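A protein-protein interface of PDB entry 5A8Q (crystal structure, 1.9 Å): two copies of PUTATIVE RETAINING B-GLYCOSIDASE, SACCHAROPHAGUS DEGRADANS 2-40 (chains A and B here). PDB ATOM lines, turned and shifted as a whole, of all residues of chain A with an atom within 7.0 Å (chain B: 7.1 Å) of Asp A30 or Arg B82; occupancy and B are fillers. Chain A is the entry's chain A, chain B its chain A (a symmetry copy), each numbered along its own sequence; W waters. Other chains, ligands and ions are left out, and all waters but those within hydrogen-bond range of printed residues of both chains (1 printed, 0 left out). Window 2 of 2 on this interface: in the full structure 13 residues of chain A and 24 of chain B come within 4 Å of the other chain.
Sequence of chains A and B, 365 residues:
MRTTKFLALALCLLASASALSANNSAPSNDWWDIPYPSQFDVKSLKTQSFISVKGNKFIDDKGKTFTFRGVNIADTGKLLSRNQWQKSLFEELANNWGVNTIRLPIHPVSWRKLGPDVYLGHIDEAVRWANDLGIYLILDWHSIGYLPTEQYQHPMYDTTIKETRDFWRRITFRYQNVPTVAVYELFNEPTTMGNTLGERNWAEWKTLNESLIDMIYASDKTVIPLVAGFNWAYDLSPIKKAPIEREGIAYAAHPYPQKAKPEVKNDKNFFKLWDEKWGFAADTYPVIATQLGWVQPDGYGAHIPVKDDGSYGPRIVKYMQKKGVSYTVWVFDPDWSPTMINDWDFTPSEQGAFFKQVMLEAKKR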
ATOM      1  N   ASN A  29      10.446 -20.938 -20.129  1.00  0.00           N
ATOM      2  CA  ASN A  29      10.112 -20.613 -18.706  1.00  0.00           C
ATOM      3  C   ASN A  29       8.589 -20.482 -18.478  1.00  0.00           C
ATOM      4  O   ASN A  29       7.939 -21.427 -18.012  1.00  0.00           O
ATOM      5  CB  ASN A  29      10.864 -19.348 -18.272  1.00  0.00           C
ATOM      6  CG  ASN A  29      10.800 -19.112 -16.778  1.00  0.00           C
ATOM      7  OD1 ASN A  29      10.685 -20.060 -15.997  1.00  0.00           O
ATOM      8  ND2 ASN A  29      10.889 -17.842 -16.367  1.00  0.00           N
ATOM      9  N   ASP A  30       8.031 -19.316 -18.795  1.00  0.00           N
ATOM     10  CA  ASP A  30       6.599 -19.097 -18.727  1.00  0.00           C
ATOM     11  C   ASP A  30       6.052 -19.323 -20.124  1.00  0.00           C
ATOM     12  O   ASP A  30       6.472 -18.656 -21.066  1.00  0.00           O
ATOM     13  CB  ASP A  30       6.294 -17.685 -18.266  1.00  0.00           C
ATOM     14  CG  ASP A  30       6.751 -17.430 -16.844  1.00  0.00           C
ATOM     15  OD1 ASP A  30       6.584 -18.329 -16.007  1.00  0.00           O
ATOM     16  OD2 ASP A  30       7.287 -16.343 -16.583  1.00  0.00           O
ATOM     17  N   TRP A  31       5.117 -20.262 -20.250  1.00  0.00           N
ATOM     18  CA  TRP A  31       4.624 -20.675 -21.559  1.00  0.00           C
ATOM     19  C   TRP A  31       4.022 -19.543 -22.380  1.00  0.00           C
ATOM     20  O   TRP A  31       4.055 -19.602 -23.602  1.00  0.00           O
ATOM     21  CB  TRP A  31       3.626 -21.846 -21.455  1.00  0.00           C
ATOM     22  CG  TRP A  31       2.611 -21.702 -20.360  1.00  0.00           C
ATOM     23  CD1 TRP A  31       2.649 -22.284 -19.132  1.00  0.00           C
ATOM     24  CD2 TRP A  31       1.401 -20.942 -20.411  1.00  0.00           C
ATOM     25  NE1 TRP A  31       1.531 -21.933 -18.401  1.00  0.00           N
ATOM     26  CE2 TRP A  31       0.748 -21.107 -19.168  1.00  0.00           C
ATOM     27  CE3 TRP A  31       0.793 -20.157 -21.394  1.00  0.00           C
ATOM     28  CZ2 TRP A  31      -0.471 -20.498 -18.873  1.00  0.00           C
ATOM     29  CZ3 TRP A  31      -0.424 -19.535 -21.094  1.00  0.00           C
ATOM     30  CH2 TRP A  31      -1.042 -19.717 -19.852  1.00  0.00           C
ATOM     31  N   TRP A  32       3.487 -18.521 -21.724  1.00  0.00           N
ATOM     32  CA  TRP A  32       2.890 -17.377 -22.447  1.00  0.00           C
ATOM     33  C   TRP A  32       3.953 -16.500 -23.120  1.00  0.00           C
ATOM     34  O   TRP A  32       3.620 -15.714 -24.006  1.00  0.00           O
ATOM     35  CB  TRP A  32       1.966 -16.517 -21.561  1.00  0.00           C
ATOM     36  CG  TRP A  32       2.592 -15.966 -20.332  1.00  0.00           C
ATOM     37  CD1 TRP A  32       3.181 -14.740 -20.187  1.00  0.00           C
ATOM     38  CD2 TRP A  32       2.672 -16.604 -19.054  1.00  0.00           C
ATOM     39  NE1 TRP A  32       3.635 -14.588 -18.901  1.00  0.00           N
ATOM     40  CE2 TRP A  32       3.352 -15.721 -18.189  1.00  0.00           C
ATOM     41  CE3 TRP A  32       2.262 -17.845 -18.561  1.00  0.00           C
ATOM     42  CZ2 TRP A  32       3.616 -16.037 -16.856  1.00  0.00           C
ATOM     43  CZ3 TRP A  32       2.528 -18.158 -17.231  1.00  0.00           C
ATOM     44  CH2 TRP A  32       3.214 -17.268 -16.405  1.00  0.00           C
ATOM     45  N   ASP A  33       5.215 -16.660 -22.733  1.00  0.00           N
ATOM     46  CA  ASP A  33       6.317 -15.915 -23.360  1.00  0.00           C
ATOM     47  C   ASP A  33       7.064 -16.690 -24.448  1.00  0.00           C
ATOM     48  O   ASP A  33       8.039 -16.182 -24.994  1.00  0.00           O
ATOM     49  CB  ASP A  33       7.320 -15.450 -22.288  1.00  0.00           C
ATOM     50  CG  ASP A  33       6.774 -14.364 -21.407  1.00  0.00           C
ATOM     51  OD1 ASP A  33       5.921 -13.571 -21.856  1.00  0.00           O
ATOM     52  OD2 ASP A  33       7.192 -14.306 -20.239  1.00  0.00           O
ATOM     53  N   ILE A  34       6.617 -17.899 -24.778  1.00  0.00           N
ATOM     54  CA  ILE A  34       7.263 -18.684 -25.839  1.00  0.00           C
ATOM     55  C   ILE A  34       7.090 -17.937 -27.169  1.00  0.00           C
ATOM     56  O   ILE A  34       5.968 -17.607 -27.541  1.00  0.00           O
ATOM     57  CB  ILE A  34       6.659 -20.090 -25.949  1.00  0.00           C
ATOM     58  CG1 ILE A  34       7.004 -20.908 -24.693  1.00  0.00           C
ATOM     59  CG2 ILE A  34       7.178 -20.826 -27.188  1.00  0.00           C
ATOM     60  CD1 ILE A  34       6.220 -22.204 -24.620  1.00  0.00           C
ATOM     61  N   GLY B  77      -2.901 -20.993 -13.819  1.00  0.00           N
ATOM     62  CA  GLY B  77      -1.491 -21.310 -13.652  1.00  0.00           C
ATOM     63  C   GLY B  77      -0.601 -20.086 -13.717  1.00  0.00           C
ATOM     64  O   GLY B  77       0.374 -19.982 -12.975  1.00  0.00           O
ATOM     65  N   LYS B  78      -0.941 -19.146 -14.591  1.00  0.00           N
ATOM     66  CA  LYS B  78      -0.202 -17.898 -14.676  1.00  0.00           C
ATOM     67  C   LYS B  78      -0.282 -17.164 -13.331  1.00  0.00           C
ATOM     68  O   LYS B  78       0.732 -16.706 -12.779  1.00  0.00           O
ATOM     69  CB  LYS B  78      -0.747 -17.058 -15.839  1.00  0.00           C
ATOM     70  CG  LYS B  78      -0.003 -15.772 -16.122  1.00  0.00           C
ATOM     71  CD  LYS B  78      -0.464 -14.619 -15.252  1.00  0.00           C
ATOM     72  CE  LYS B  78       0.184 -13.299 -15.676  1.00  0.00           C
ATOM     73  NZ  LYS B  78      -0.160 -12.244 -14.688  1.00  0.00           N
ATOM     74  N   LEU B  79      -1.489 -17.063 -12.786  1.00  0.00           N
ATOM     75  CA  LEU B  79      -1.688 -16.370 -11.522  1.00  0.00           C
ATOM     76  C   LEU B  79      -1.009 -17.068 -10.339  1.00  0.00           C
ATOM     77  O   LEU B  79      -0.390 -16.409  -9.481  1.00  0.00           O
ATOM     78  CB  LEU B  79      -3.179 -16.169 -11.259  1.00  0.00           C
ATOM     79  CG  LEU B  79      -3.838 -15.185 -12.235  1.00  0.00           C
ATOM     80  CD1 LEU B  79      -5.347 -15.244 -12.168  1.00  0.00           C
ATOM     81  CD2 LEU B  79      -3.357 -13.776 -11.942  1.00  0.00           C
ATOM     82  N   LEU B  80      -1.130 -18.396 -10.294  1.00  0.00           N
ATOM     83  CA  LEU B  80      -0.475 -19.182  -9.261  1.00  0.00           C
ATOM     84  C   LEU B  80       1.035 -18.961  -9.234  1.00  0.00           C
ATOM     85  O   LEU B  80       1.617 -18.874  -8.165  1.00  0.00           O
ATOM     86  CB  LEU B  80      -0.756 -20.672  -9.454  1.00  0.00           C
ATOM     87  CG  LEU B  80      -2.150 -21.107  -9.021  1.00  0.00           C
ATOM     88  CD1 LEU B  80      -2.474 -22.465  -9.622  1.00  0.00           C
ATOM     89  CD2 LEU B  80      -2.237 -21.142  -7.494  1.00  0.00           C
ATOM     90  N   SER B  81       1.659 -18.843 -10.404  1.00  0.00           N
ATOM     91  CA  SER B  81       3.122 -18.741 -10.489  1.00  0.00           C
ATOM     92  C   SER B  81       3.662 -17.506  -9.760  1.00  0.00           C
ATOM     93  O   SER B  81       4.819 -17.502  -9.325  1.00  0.00           O
ATOM     94  CB  SER B  81       3.606 -18.732 -11.951  1.00  0.00           C
ATOM     95  OG  SER B  81       3.310 -17.488 -12.568  1.00  0.00           O
ATOM     96  N   ARG B  82       2.837 -16.467  -9.620  1.00  0.00           N
ATOM     97  CA  ARG B  82       3.229 -15.260  -8.876  1.00  0.00           C
ATOM     98  C   ARG B  82       2.388 -15.048  -7.599  1.00  0.00           C
ATOM     99  O   ARG B  82       2.336 -13.940  -7.069  1.00  0.00           O
ATOM    100  CB  ARG B  82       3.121 -14.016  -9.768  1.00  0.00           C
ATOM    101  CG  ARG B  82       3.760 -14.129 -11.153  1.00  0.00           C
ATOM    102  CD  ARG B  82       5.232 -14.499 -11.100  1.00  0.00           C
ATOM    103  NE  ARG B  82       5.977 -14.138 -12.321  1.00  0.00           N
ATOM    104  CZ  ARG B  82       6.100 -14.887 -13.425  1.00  0.00           C
ATOM    105  NH1 ARG B  82       5.513 -16.076 -13.544  1.00  0.00           N
ATOM    106  NH2 ARG B  82       6.830 -14.427 -14.437  1.00  0.00           N
ATOM    107  N   ASN B  83       1.734 -16.107  -7.135  1.00  0.00           N
ATOM    108  CA  ASN B  83       0.915 -16.069  -5.918  1.00  0.00           C
ATOM    109  C   ASN B  83      -0.221 -15.053  -6.008  1.00  0.00           C
ATOM    110  O   ASN B  83      -0.584 -14.407  -5.023  1.00  0.00           O
ATOM    111  CB  ASN B  83       1.795 -15.808  -4.692  1.00  0.00           C
ATOM    112  CG  ASN B  83       2.937 -16.802  -4.578  1.00  0.00           C
ATOM    113  OD1 ASN B  83       2.717 -18.013  -4.531  1.00  0.00           O
ATOM    114  ND2 ASN B  83       4.163 -16.296  -4.519  1.00  0.00           N
ATOM    115  N   GLN B  84      -0.796 -14.919  -7.203  1.00  0.00           N
ATOM    116  CA  GLN B  84      -1.902 -13.989  -7.416  1.00  0.00           C
ATOM    117  C   GLN B  84      -3.245 -14.704  -7.572  1.00  0.00           C
ATOM    118  O   GLN B  84      -4.257 -14.067  -7.836  1.00  0.00           O
ATOM    119  CB  GLN B  84      -1.634 -13.111  -8.639  1.00  0.00           C
ATOM    120  CG  GLN B  84      -0.419 -12.203  -8.507  1.00  0.00           C
ATOM    121  CD  GLN B  84      -0.580 -11.136  -7.443  1.00  0.00           C
ATOM    122  OE1 GLN B  84      -1.693 -10.798  -7.042  1.00  0.00           O
ATOM    123  NE2 GLN B  84       0.538 -10.595  -6.982  1.00  0.00           N
ATOM    124  N   TRP B  85      -3.252 -16.026  -7.411  1.00  0.00           N
ATOM    125  CA  TRP B  85      -4.501 -16.791  -7.422  1.00  0.00           C
ATOM    126  C   TRP B  85      -5.061 -16.770  -6.017  1.00  0.00           C
ATOM    127  O   TRP B  85      -4.727 -17.620  -5.199  1.00  0.00           O
ATOM    128  CB  TRP B  85      -4.266 -18.224  -7.887  1.00  0.00           C
ATOM    129  CG  TRP B  85      -5.516 -19.027  -8.005  1.00  0.00           C
ATOM    130  CD1 TRP B  85      -5.914 -20.041  -7.178  1.00  0.00           C
ATOM    131  CD2 TRP B  85      -6.543 -18.890  -8.994  1.00  0.00           C
ATOM    132  NE1 TRP B  85      -7.114 -20.550  -7.598  1.00  0.00           N
ATOM    133  CE2 TRP B  85      -7.531 -19.859  -8.703  1.00  0.00           C
ATOM    134  CE3 TRP B  85      -6.719 -18.063 -10.105  1.00  0.00           C
ATOM    135  CZ2 TRP B  85      -8.689 -20.011  -9.479  1.00  0.00           C
ATOM    136  CZ3 TRP B  85      -7.869 -18.215 -10.879  1.00  0.00           C
ATOM    137  CH2 TRP B  85      -8.836 -19.188 -10.557  1.00  0.00           C
ATOM    138  N   GLN B  86      -5.911 -15.784  -5.749  1.00  0.00           N
ATOM    139  CA  GLN B  86      -6.381 -15.456  -4.401  1.00  0.00           C
ATOM    140  C   GLN B  86      -7.818 -14.945  -4.440  1.00  0.00           C
ATOM    141  O   GLN B  86      -8.193 -14.286  -5.402  1.00  0.00           O
ATOM    142  CB  GLN B  86      -5.522 -14.327  -3.818  1.00  0.00           C
ATOM    143  CG  GLN B  86      -4.024 -14.593  -3.789  1.00  0.00           C
ATOM    144  CD  GLN B  86      -3.618 -15.597  -2.731  1.00  0.00           C
ATOM    145  OE1 GLN B  86      -4.437 -16.018  -1.910  1.00  0.00           O
ATOM    146  NE2 GLN B  86      -2.344 -15.985  -2.738  1.00  0.00           N
ATOM    147  N   LYS B 113       0.219 -28.747 -17.752  1.00  0.00           N
ATOM    148  CA  LYS B 113       1.311 -28.462 -16.841  1.00  0.00           C
ATOM    149  C   LYS B 113       0.939 -28.695 -15.369  1.00  0.00           C
ATOM    150  O   LYS B 113       1.671 -29.362 -14.650  1.00  0.00           O
ATOM    151  CB  LYS B 113       1.832 -27.053 -17.046  1.00  0.00           C
ATOM    152  CG  LYS B 113       3.147 -26.818 -16.322  1.00  0.00           C
ATOM    153  CD  LYS B 113       3.786 -25.509 -16.723  1.00  0.00           C
ATOM    154  CE  LYS B 113       5.149 -25.357 -16.062  1.00  0.00           C
ATOM    155  NZ  LYS B 113       5.760 -24.086 -16.517  1.00  0.00           N
ATOM    156  N   ASP B 335      -0.067  -7.826 -16.752  1.00  0.00           N
ATOM    157  CA  ASP B 335       0.993  -8.339 -17.642  1.00  0.00           C
ATOM    158  C   ASP B 335       0.457  -8.659 -19.037  1.00  0.00           C
ATOM    159  O   ASP B 335       1.073  -8.330 -20.031  1.00  0.00           O
ATOM    160  CB  ASP B 335       1.620  -9.609 -17.053  1.00  0.00           C
ATOM    161  CG  ASP B 335       2.142  -9.402 -15.648  1.00  0.00           C
ATOM    162  OD1 ASP B 335       2.902  -8.445 -15.449  1.00  0.00           O
ATOM    163  OD2 ASP B 335       1.785 -10.190 -14.744  1.00  0.00           O
ATOM    164  N   TRP B 344      -0.749  -4.725  -9.505  1.00  0.00           N
ATOM    165  CA  TRP B 344      -1.600  -5.519  -8.627  1.00  0.00           C
ATOM    166  C   TRP B 344      -2.255  -4.724  -7.503  1.00  0.00           C
ATOM    167  O   TRP B 344      -2.991  -5.297  -6.698  1.00  0.00           O
ATOM    168  CB  TRP B 344      -0.855  -6.745  -8.105  1.00  0.00           C
ATOM    169  CG  TRP B 344      -0.762  -7.833  -9.153  1.00  0.00           C
ATOM    170  CD1 TRP B 344       0.368  -8.349  -9.703  1.00  0.00           C
ATOM    171  CD2 TRP B 344      -1.858  -8.504  -9.787  1.00  0.00           C
ATOM    172  NE1 TRP B 344       0.048  -9.329 -10.614  1.00  0.00           N
ATOM    173  CE2 TRP B 344      -1.313  -9.432 -10.691  1.00  0.00           C
ATOM    174  CE3 TRP B 344      -3.246  -8.412  -9.669  1.00  0.00           C
ATOM    175  CZ2 TRP B 344      -2.109 -10.272 -11.475  1.00  0.00           C
ATOM    176  CZ3 TRP B 344      -4.039  -9.245 -10.448  1.00  0.00           C
ATOM    177  CH2 TRP B 344      -3.466 -10.158 -11.342  1.00  0.00           C
HETATM  178  O   HOH W   1       5.205 -21.493 -17.332  1.00  0.00           O
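O of Lys B78 sits at hydrogen-bond distance from OG of Ser B81, at 2.7 Å.
OD2 of Asp B335 is in salt-bridge range of NZ of Lys B78 (2.8 Å).
The guanidinium group (NH1) of Arg B82 lies within hydrogen-bond range of the side-chain hydroxyl (OG) of Ser B81 (2.8 Å).
Among the printed residues, pairs that only touch across the chains: Trp A32 with Lys B78 (3.6 Å), Asn A29 with Lys B113 (3.7 Å), Trp A32 with Arg B82 (3.8 Å) and Trp A32 with Ser B81 (3.8 Å).
Of the printed residues of chain B, Asn A29 touches Lys B113.
Of the printed residues of chain B, Asp A30 touches Arg B82 (2.9 Å).
Of the printed residues of chain A, Lys B78 touches Trp A32.
Printed residues of chain A within 4 Å of Ser B81: Trp A32 (3.8 Å).
Printed residues of chain A within 4 Å of Arg B82: Asp A30 (2.9 Å) and Trp A32 (3.8 Å).
Printed residues of chain A within 4 Å of Lys B113: Asn A29.
The nearest printed residue of chain B that does not touch Trp A32 is Gly B77 (5.1 Å).
No position is printed for both chains.
Of the 5 pairs that touch across the chains among the printed residues, none has its exchanged pair printed and touching as well.
The side-chain carboxylate (OD2) of Asp A30 is in salt-bridge range of the guanidinium group (NH2) of Arg B82 (2.9 Å).
Of the 13 printed residues of chain B, 4 touch a printed residue of chain A.
Of the 6 printed residues of chain A, 3 touch a printed residue of chain B.
Printed residues of chain A that touch a printed residue of chain B: Asn A29, Asp A30 and Trp A32.
Among the printed residues, Asp or Glu carboxylates within 4 Å of a Lys or Arg side-chain nitrogen of the other chain: Asp A30 with Arg B82 (2.9 Å).
Water W1 lies within hydrogen-bond range of the side-chain amino group of Lys B113, the backbone carbonyl oxygen of Asn A29 and the backbone NH of Trp A31.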
